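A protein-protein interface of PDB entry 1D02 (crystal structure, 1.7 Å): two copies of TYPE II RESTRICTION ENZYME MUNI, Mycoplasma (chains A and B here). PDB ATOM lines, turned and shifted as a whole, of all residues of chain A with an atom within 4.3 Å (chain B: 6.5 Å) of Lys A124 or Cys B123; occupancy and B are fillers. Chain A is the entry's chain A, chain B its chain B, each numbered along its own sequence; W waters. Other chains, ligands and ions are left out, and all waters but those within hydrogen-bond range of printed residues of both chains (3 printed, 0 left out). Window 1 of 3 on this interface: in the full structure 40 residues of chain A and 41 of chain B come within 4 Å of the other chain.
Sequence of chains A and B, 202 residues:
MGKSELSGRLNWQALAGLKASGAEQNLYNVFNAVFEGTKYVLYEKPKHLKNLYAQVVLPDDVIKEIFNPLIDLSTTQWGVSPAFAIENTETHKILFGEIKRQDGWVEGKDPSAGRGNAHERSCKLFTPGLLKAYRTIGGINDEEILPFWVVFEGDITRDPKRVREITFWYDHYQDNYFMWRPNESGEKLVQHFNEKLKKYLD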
ATOM      1  N   VAL A  80      35.668   0.372 -35.707  1.00  0.00           N
ATOM      2  CA  VAL A  80      34.404   0.925 -36.187  1.00  0.00           C
ATOM      3  C   VAL A  80      34.577   1.653 -37.504  1.00  0.00           C
ATOM      4  O   VAL A  80      35.701   1.970 -37.900  1.00  0.00           O
ATOM      5  CB  VAL A  80      33.778   1.885 -35.173  1.00  0.00           C
ATOM      6  CG1 VAL A  80      33.456   1.136 -33.864  1.00  0.00           C
ATOM      7  CG2 VAL A  80      34.720   3.057 -34.913  1.00  0.00           C
ATOM      8  N   ARG A 121      21.493   3.085 -30.982  1.00  0.00           N
ATOM      9  CA  ARG A 121      22.797   2.508 -31.320  1.00  0.00           C
ATOM     10  C   ARG A 121      23.884   3.593 -31.405  1.00  0.00           C
ATOM     11  O   ARG A 121      25.050   3.344 -31.079  1.00  0.00           O
ATOM     12  CB  ARG A 121      22.725   1.777 -32.681  1.00  0.00           C
ATOM     13  CG  ARG A 121      21.928   0.444 -32.682  1.00  0.00           C
ATOM     14  CD  ARG A 121      21.911  -0.211 -34.099  1.00  0.00           C
ATOM     15  NE  ARG A 121      23.247  -0.043 -34.607  1.00  0.00           N
ATOM     16  CZ  ARG A 121      23.598   0.594 -35.726  1.00  0.00           C
ATOM     17  NH1 ARG A 121      22.721   1.131 -36.578  1.00  0.00           N
ATOM     18  NH2 ARG A 121      24.884   0.855 -35.887  1.00  0.00           N
ATOM     19  N   SER A 122      23.515   4.791 -31.849  1.00  0.00           N
ATOM     20  CA  SER A 122      24.510   5.861 -31.985  1.00  0.00           C
ATOM     21  C   SER A 122      25.106   6.273 -30.645  1.00  0.00           C
ATOM     22  O   SER A 122      26.149   6.928 -30.594  1.00  0.00           O
ATOM     23  CB  SER A 122      23.901   7.099 -32.670  1.00  0.00           C
ATOM     24  OG  SER A 122      22.783   7.612 -31.951  1.00  0.00           O
ATOM     25  N   CYS A 123      24.455   5.896 -29.558  1.00  0.00           N
ATOM     26  CA  CYS A 123      24.965   6.286 -28.256  1.00  0.00           C
ATOM     27  C   CYS A 123      26.242   5.539 -27.884  1.00  0.00           C
ATOM     28  O   CYS A 123      26.841   5.848 -26.856  1.00  0.00           O
ATOM     29  CB  CYS A 123      23.902   6.090 -27.168  1.00  0.00           C
ATOM     30  SG  CYS A 123      22.520   7.249 -27.338  1.00  0.00           S
ATOM     31  N   LYS A 124      26.644   4.561 -28.697  1.00  0.00           N
ATOM     32  CA  LYS A 124      27.895   3.856 -28.430  1.00  0.00           C
ATOM     33  C   LYS A 124      29.047   4.883 -28.408  1.00  0.00           C
ATOM     34  O   LYS A 124      30.098   4.641 -27.781  1.00  0.00           O
ATOM     35  CB  LYS A 124      28.171   2.797 -29.505  1.00  0.00           C
ATOM     36  CG  LYS A 124      28.525   3.372 -30.879  1.00  0.00           C
ATOM     37  CD  LYS A 124      28.573   2.251 -31.928  1.00  0.00           C
ATOM     38  CE  LYS A 124      29.820   1.347 -31.835  1.00  0.00           C
ATOM     39  NZ  LYS A 124      29.880   0.391 -33.025  1.00  0.00           N
ATOM     40  N   LEU A 125      28.845   6.030 -29.052  1.00  0.00           N
ATOM     41  CA  LEU A 125      29.887   7.068 -29.080  1.00  0.00           C
ATOM     42  C   LEU A 125      30.120   7.762 -27.741  1.00  0.00           C
ATOM     43  O   LEU A 125      31.141   8.433 -27.571  1.00  0.00           O
ATOM     44  CB  LEU A 125      29.595   8.101 -30.187  1.00  0.00           C
ATOM     45  CG  LEU A 125      29.592   7.434 -31.571  1.00  0.00           C
ATOM     46  CD1 LEU A 125      29.416   8.459 -32.666  1.00  0.00           C
ATOM     47  CD2 LEU A 125      30.904   6.649 -31.778  1.00  0.00           C
ATOM     48  N   PHE A 126      29.185   7.602 -26.803  1.00  0.00           N
ATOM     49  CA  PHE A 126      29.314   8.161 -25.459  1.00  0.00           C
ATOM     50  C   PHE A 126      30.076   7.199 -24.525  1.00  0.00           C
ATOM     51  O   PHE A 126      30.378   7.559 -23.377  1.00  0.00           O
ATOM     52  CB  PHE A 126      27.936   8.444 -24.829  1.00  0.00           C
ATOM     53  CG  PHE A 126      27.217   9.617 -25.433  1.00  0.00           C
ATOM     54  CD1 PHE A 126      26.275   9.427 -26.438  1.00  0.00           C
ATOM     55  CD2 PHE A 126      27.473  10.912 -24.999  1.00  0.00           C
ATOM     56  CE1 PHE A 126      25.593  10.501 -26.991  1.00  0.00           C
ATOM     57  CE2 PHE A 126      26.788  11.995 -25.557  1.00  0.00           C
ATOM     58  CZ  PHE A 126      25.851  11.781 -26.552  1.00  0.00           C
ATOM     59  N   THR A 127      30.397   5.991 -24.982  1.00  0.00           N
ATOM     60  CA  THR A 127      31.127   5.084 -24.076  1.00  0.00           C
ATOM     61  C   THR A 127      32.515   5.666 -23.820  1.00  0.00           C
ATOM     62  O   THR A 127      33.142   6.248 -24.720  1.00  0.00           O
ATOM     63  CB  THR A 127      31.333   3.665 -24.659  1.00  0.00           C
ATOM     64  OG1 THR A 127      32.081   3.747 -25.883  1.00  0.00           O
ATOM     65  CG2 THR A 127      29.977   2.966 -24.890  1.00  0.00           C
ATOM     66  N   LEU A 130      35.216   4.587 -26.521  1.00  0.00           N
ATOM     67  CA  LEU A 130      35.187   5.209 -27.828  1.00  0.00           C
ATOM     68  C   LEU A 130      35.469   6.716 -27.739  1.00  0.00           C
ATOM     69  O   LEU A 130      36.067   7.297 -28.661  1.00  0.00           O
ATOM     70  CB  LEU A 130      33.857   4.893 -28.534  1.00  0.00           C
ATOM     71  CG  LEU A 130      33.762   3.426 -29.029  1.00  0.00           C
ATOM     72  CD1 LEU A 130      32.403   3.138 -29.689  1.00  0.00           C
ATOM     73  CD2 LEU A 130      34.894   3.147 -30.009  1.00  0.00           C
ATOM     74  N   ASN B 117      24.532  -5.910 -34.231  1.00  0.00           N
ATOM     75  CA  ASN B 117      24.945  -4.715 -33.490  1.00  0.00           C
ATOM     76  C   ASN B 117      23.851  -4.050 -32.669  1.00  0.00           C
ATOM     77  O   ASN B 117      24.050  -2.956 -32.149  1.00  0.00           O
ATOM     78  CB  ASN B 117      25.547  -3.671 -34.457  1.00  0.00           C
ATOM     79  CG  ASN B 117      24.569  -3.251 -35.550  1.00  0.00           C
ATOM     80  OD1 ASN B 117      23.475  -3.789 -35.657  1.00  0.00           O
ATOM     81  ND2 ASN B 117      24.979  -2.292 -36.379  1.00  0.00           N
ATOM     82  N   HIS B 119      22.992  -4.649 -29.794  1.00  0.00           N
ATOM     83  CA  HIS B 119      23.426  -4.483 -28.394  1.00  0.00           C
ATOM     84  C   HIS B 119      23.952  -3.081 -28.129  1.00  0.00           C
ATOM     85  O   HIS B 119      24.045  -2.641 -26.971  1.00  0.00           O
ATOM     86  CB  HIS B 119      24.517  -5.495 -27.999  1.00  0.00           C
ATOM     87  CG  HIS B 119      25.772  -5.388 -28.814  1.00  0.00           C
ATOM     88  ND1 HIS B 119      25.794  -5.604 -30.174  1.00  0.00           N
ATOM     89  CD2 HIS B 119      27.054  -5.135 -28.447  1.00  0.00           C
ATOM     90  CE1 HIS B 119      27.039  -5.487 -30.612  1.00  0.00           C
ATOM     91  NE2 HIS B 119      27.822  -5.205 -29.584  1.00  0.00           N
ATOM     92  N   GLU B 120      24.325  -2.390 -29.193  1.00  0.00           N
ATOM     93  CA  GLU B 120      24.810  -1.014 -29.046  1.00  0.00           C
ATOM     94  C   GLU B 120      23.760  -0.099 -28.406  1.00  0.00           C
ATOM     95  O   GLU B 120      24.099   0.933 -27.826  1.00  0.00           O
ATOM     96  CB  GLU B 120      25.191  -0.434 -30.411  1.00  0.00           C
ATOM     97  CG  GLU B 120      26.424  -1.107 -31.030  1.00  0.00           C
ATOM     98  CD  GLU B 120      26.637  -0.701 -32.502  1.00  0.00           C
ATOM     99  OE1 GLU B 120      25.766   0.003 -33.075  1.00  0.00           O
ATOM    100  OE2 GLU B 120      27.667  -1.106 -33.076  1.00  0.00           O
ATOM    101  N   ARG B 121      22.484  -0.458 -28.543  1.00  0.00           N
ATOM    102  CA  ARG B 121      21.397   0.353 -27.979  1.00  0.00           C
ATOM    103  C   ARG B 121      21.565   0.565 -26.465  1.00  0.00           C
ATOM    104  O   ARG B 121      21.126   1.583 -25.921  1.00  0.00           O
ATOM    105  CB  ARG B 121      20.029  -0.323 -28.223  1.00  0.00           C
ATOM    106  CG  ARG B 121      19.621  -0.482 -29.725  1.00  0.00           C
ATOM    107  CD  ARG B 121      18.307  -1.258 -29.840  1.00  0.00           C
ATOM    108  NE  ARG B 121      17.522  -0.814 -28.736  1.00  0.00           N
ATOM    109  CZ  ARG B 121      16.962  -1.575 -27.800  1.00  0.00           C
ATOM    110  NH1 ARG B 121      16.997  -2.896 -27.812  1.00  0.00           N
ATOM    111  NH2 ARG B 121      16.543  -0.974 -26.705  1.00  0.00           N
ATOM    112  N   SER B 122      22.186  -0.409 -25.803  1.00  0.00           N
ATOM    113  CA  SER B 122      22.383  -0.337 -24.363  1.00  0.00           C
ATOM    114  C   SER B 122      23.245   0.843 -24.001  1.00  0.00           C
ATOM    115  O   SER B 122      23.175   1.339 -22.872  1.00  0.00           O
ATOM    116  CB  SER B 122      23.013  -1.630 -23.819  1.00  0.00           C
ATOM    117  OG  SER B 122      24.284  -1.875 -24.381  1.00  0.00           O
ATOM    118  N   CYS B 123      24.024   1.331 -24.962  1.00  0.00           N
ATOM    119  CA  CYS B 123      24.916   2.458 -24.674  1.00  0.00           C
ATOM    120  C   CYS B 123      24.184   3.775 -24.428  1.00  0.00           C
ATOM    121  O   CYS B 123      24.823   4.769 -24.083  1.00  0.00           O
ATOM    122  CB  CYS B 123      25.962   2.637 -25.782  1.00  0.00           C
ATOM    123  SG  CYS B 123      27.134   1.258 -25.877  1.00  0.00           S
ATOM    124  N   LYS B 124      22.864   3.796 -24.608  1.00  0.00           N
ATOM    125  CA  LYS B 124      22.115   5.016 -24.314  1.00  0.00           C
ATOM    126  C   LYS B 124      22.329   5.397 -22.844  1.00  0.00           C
ATOM    127  O   LYS B 124      22.202   6.569 -22.475  1.00  0.00           O
ATOM    128  CB  LYS B 124      20.625   4.813 -24.546  1.00  0.00           C
ATOM    129  CG  LYS B 124      19.968   3.772 -23.633  1.00  0.00           C
ATOM    130  CD  LYS B 124      18.537   3.441 -24.085  1.00  0.00           C
ATOM    131  CE  LYS B 124      17.585   4.642 -23.999  1.00  0.00           C
ATOM    132  NZ  LYS B 124      16.121   4.260 -24.252  1.00  0.00           N
ATOM    133  N   LEU B 125      22.672   4.415 -22.021  1.00  0.00           N
ATOM    134  CA  LEU B 125      22.854   4.676 -20.594  1.00  0.00           C
ATOM    135  C   LEU B 125      24.094   5.518 -20.328  1.00  0.00           C
ATOM    136  O   LEU B 125      24.243   6.045 -19.234  1.00  0.00           O
ATOM    137  CB  LEU B 125      22.935   3.360 -19.820  1.00  0.00           C
ATOM    138  CG  LEU B 125      21.684   2.486 -19.943  1.00  0.00           C
ATOM    139  CD1 LEU B 125      21.884   1.186 -19.181  1.00  0.00           C
ATOM    140  CD2 LEU B 125      20.470   3.252 -19.424  1.00  0.00           C
ATOM    141  N   PHE B 126      24.974   5.631 -21.319  1.00  0.00           N
ATOM    142  CA  PHE B 126      26.177   6.455 -21.164  1.00  0.00           C
ATOM    143  C   PHE B 126      25.938   7.929 -21.533  1.00  0.00           C
ATOM    144  O   PHE B 126      26.841   8.767 -21.353  1.00  0.00           O
ATOM    145  CB  PHE B 126      27.329   5.925 -22.030  1.00  0.00           C
ATOM    146  CG  PHE B 126      27.904   4.612 -21.562  1.00  0.00           C
ATOM    147  CD1 PHE B 126      27.452   3.406 -22.075  1.00  0.00           C
ATOM    148  CD2 PHE B 126      28.960   4.588 -20.657  1.00  0.00           C
ATOM    149  CE1 PHE B 126      28.056   2.190 -21.698  1.00  0.00           C
ATOM    150  CE2 PHE B 126      29.550   3.392 -20.287  1.00  0.00           C
ATOM    151  CZ  PHE B 126      29.098   2.195 -20.813  1.00  0.00           C
ATOM    152  N   THR B 127      24.752   8.259 -22.065  1.00  0.00           N
ATOM    153  CA  THR B 127      24.493   9.664 -22.413  1.00  0.00           C
ATOM    154  C   THR B 127      24.512  10.495 -21.142  1.00  0.00           C
ATOM    155  O   THR B 127      24.074  10.039 -20.080  1.00  0.00           O
ATOM    156  CB  THR B 127      23.120   9.870 -23.100  1.00  0.00           C
ATOM    157  OG1 THR B 127      22.056   9.390 -22.266  1.00  0.00           O
ATOM    158  CG2 THR B 127      23.113   9.136 -24.449  1.00  0.00           C
ATOM    159  N   PHE B 148      24.304   2.140 -13.568  1.00  0.00           N
ATOM    160  CA  PHE B 148      23.546   1.076 -14.219  1.00  0.00           C
ATOM    161  C   PHE B 148      24.394  -0.170 -14.355  1.00  0.00           C
ATOM    162  O   PHE B 148      25.618  -0.127 -14.190  1.00  0.00           O
ATOM    163  CB  PHE B 148      23.083   1.535 -15.611  1.00  0.00           C
ATOM    164  CG  PHE B 148      24.223   1.881 -16.543  1.00  0.00           C
ATOM    165  CD1 PHE B 148      24.830   0.889 -17.314  1.00  0.00           C
ATOM    166  CD2 PHE B 148      24.684   3.190 -16.647  1.00  0.00           C
ATOM    167  CE1 PHE B 148      25.885   1.199 -18.183  1.00  0.00           C
ATOM    168  CE2 PHE B 148      25.732   3.514 -17.508  1.00  0.00           C
ATOM    169  CZ  PHE B 148      26.342   2.530 -18.283  1.00  0.00           C
ATOM    170  N   VAL B 150      24.600  -3.544 -17.030  1.00  0.00           N
ATOM    171  CA  VAL B 150      24.101  -4.214 -18.228  1.00  0.00           C
ATOM    172  C   VAL B 150      24.562  -5.675 -18.174  1.00  0.00           C
ATOM    173  O   VAL B 150      25.753  -5.959 -18.045  1.00  0.00           O
ATOM    174  CB  VAL B 150      24.644  -3.549 -19.525  1.00  0.00           C
ATOM    175  CG1 VAL B 150      24.174  -4.332 -20.745  1.00  0.00           C
ATOM    176  CG2 VAL B 150      24.155  -2.075 -19.638  1.00  0.00           C
ATOM    177  N   GLU B 165      35.121  -5.936 -27.811  1.00  0.00           N
ATOM    178  CA  GLU B 165      34.470  -4.662 -28.131  1.00  0.00           C
ATOM    179  C   GLU B 165      33.840  -4.044 -26.873  1.00  0.00           C
ATOM    180  O   GLU B 165      34.090  -2.877 -26.528  1.00  0.00           O
ATOM    181  CB  GLU B 165      33.366  -4.903 -29.175  1.00  0.00           C
ATOM    182  CG  GLU B 165      32.376  -3.738 -29.351  1.00  0.00           C
ATOM    183  CD  GLU B 165      31.168  -4.165 -30.181  1.00  0.00           C
ATOM    184  OE1 GLU B 165      30.579  -5.233 -29.875  1.00  0.00           O
ATOM    185  OE2 GLU B 165      30.816  -3.429 -31.126  1.00  0.00           O
ATOM    186  N   TRP B 169      34.654  -0.670 -24.801  1.00  0.00           N
ATOM    187  CA  TRP B 169      33.696   0.400 -24.551  1.00  0.00           C
ATOM    188  C   TRP B 169      33.684   0.859 -23.097  1.00  0.00           C
ATOM    189  O   TRP B 169      33.696   2.053 -22.816  1.00  0.00           O
ATOM    190  CB  TRP B 169      32.261  -0.064 -24.838  1.00  0.00           C
ATOM    191  CG  TRP B 169      31.847  -0.280 -26.257  1.00  0.00           C
ATOM    192  CD1 TRP B 169      32.543   0.012 -27.408  1.00  0.00           C
ATOM    193  CD2 TRP B 169      30.606  -0.862 -26.667  1.00  0.00           C
ATOM    194  NE1 TRP B 169      31.799  -0.367 -28.515  1.00  0.00           N
ATOM    195  CE2 TRP B 169      30.610  -0.906 -28.087  1.00  0.00           C
ATOM    196  CE3 TRP B 169      29.488  -1.358 -25.968  1.00  0.00           C
ATOM    197  CZ2 TRP B 169      29.539  -1.428 -28.819  1.00  0.00           C
ATOM    198  CZ3 TRP B 169      28.413  -1.881 -26.697  1.00  0.00           C
ATOM    199  CH2 TRP B 169      28.457  -1.909 -28.115  1.00  0.00           C
ATOM    200  N   TYR B 170      33.614  -0.101 -22.174  1.00  0.00           N
ATOM    201  CA  TYR B 170      33.498   0.214 -20.755  1.00  0.00           C
ATOM    202  C   TYR B 170      34.751   0.789 -20.088  1.00  0.00           C
ATOM    203  O   TYR B 170      34.650   1.382 -19.023  1.00  0.00           O
ATOM    204  CB  TYR B 170      32.946  -1.005 -19.982  1.00  0.00           C
ATOM    205  CG  TYR B 170      31.418  -1.175 -20.125  1.00  0.00           C
ATOM    206  CD1 TYR B 170      30.853  -1.603 -21.326  1.00  0.00           C
ATOM    207  CD2 TYR B 170      30.559  -0.819 -19.077  1.00  0.00           C
ATOM    208  CE1 TYR B 170      29.453  -1.662 -21.482  1.00  0.00           C
ATOM    209  CE2 TYR B 170      29.177  -0.880 -19.211  1.00  0.00           C
ATOM    210  CZ  TYR B 170      28.632  -1.301 -20.419  1.00  0.00           C
ATOM    211  OH  TYR B 170      27.261  -1.362 -20.544  1.00  0.00           O
HETATM  212  O   HOH W   1      27.426  -0.830 -35.735  1.00  0.00           O
HETATM  213  O   HOH W   2      29.935   9.073 -21.283  1.00  0.00           O
HETATM  214  O   HOH W   3      31.861  -1.283 -32.036  1.00  0.00           O
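The side-chain amide nitrogen (ND2) of Asn B117 lies close to the guanidinium group (NH2) of Arg A121 (3.2 Å).
The guanidinium group (NE) of Arg A121 is in salt-bridge range of the side-chain carboxylate (OE1) of Glu B120 (2.9 Å).
The side-chain amino group (NZ) of Lys A124 is in salt-bridge range of the side-chain carboxylate (OE2) of Glu B120, 2.7 Å away.
O of Lys A124 lies within hydrogen-bond range of OG1 of Thr A127.
The side-chain hydroxyl (OG1) of Thr A127 lies within hydrogen-bond range of the backbone NH (N) of Leu A130.
The backbone carbonyl oxygen (O) of Glu B120 lies close to the side-chain sulfur (SG) of Cys B123, 3.6 Å away.
The side-chain hydroxyl (OG1) of Thr B127 sits at hydrogen-bond distance from the backbone carbonyl oxygen (O) of Lys B124 (2.8 Å).
Among the printed residues, pairs that only touch across the chains: Thr A127 with Trp B169 (3.4 Å), Thr A127 with Cys B123 (3.5 Å), Cys A123 with Cys B123 (3.5 Å), Lys A124 with Cys B123 (3.5 Å), Cys A123 with Thr B127 (3.5 Å), Cys A123 with Lys B124 (3.5 Å), Phe A126 with Phe B126 (3.7 Å), Leu A130 with Trp B169 (3.7 Å), Phe A126 with Thr B127 (3.7 Å), Thr A127 with Phe B126 (3.8 Å) and Arg A121 with Arg B121 (3.9 Å).
Ser A122 touches none of the printed residues of chain B.
Printed residues of chain B within 4 Å of Cys A123: Cys B123 (3.5 Å), Lys B124 (3.5 Å) and Thr B127 (3.5 Å).
Of chain B, only Glu B120 (2.7 Å) and Cys B123 (3.5 Å) come within 4 Å of Lys A124.
His B119 touches none of the printed residues of chain A.
Of the printed residues of chain A, Glu B120 touches Arg A121 (2.9 Å) and Lys A124 (2.7 Å).
Of chain A, only Cys A123 (3.5 Å), Lys A124 (3.5 Å) and Thr A127 (3.5 Å) come within 4 Å of Cys B123.
Of the printed residues of chain A, Phe B126 touches Phe A126 (3.7 Å) and Thr A127 (3.8 Å).
The nearest printed residue of chain A that does not touch Cys B123 is Phe A126 (4.9 Å).
Arg B121 touches its own counterpart, Arg A121.
Cys A123 touches its own counterpart, Cys B123.
Cys A123 touches Thr B127, and with the chains exchanged Thr A127 touches Cys B123.
Phe A126 touches its own counterpart, Phe B126.
Of the 14 pairs that touch across the chains among the printed residues, 9 have their exchanged pair printed and touching as well.
Water W3 lies within hydrogen-bond range of OE2 of Glu B165 (2.6 Å) and NZ of Lys A124 (2.8 Å).
Water W2 bridges O of Phe A126 (2.6 Å) and O of Phe B126 (3.1 Å).
Water W1 lies within hydrogen-bond range of the side-chain carboxylate (OE2) of Glu B120 (2.7 Å), the side-chain amide nitrogen (ND2) of Asn B117 (2.9 Å) and the guanidinium group (NH2) of Arg A121 (3.1 Å).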
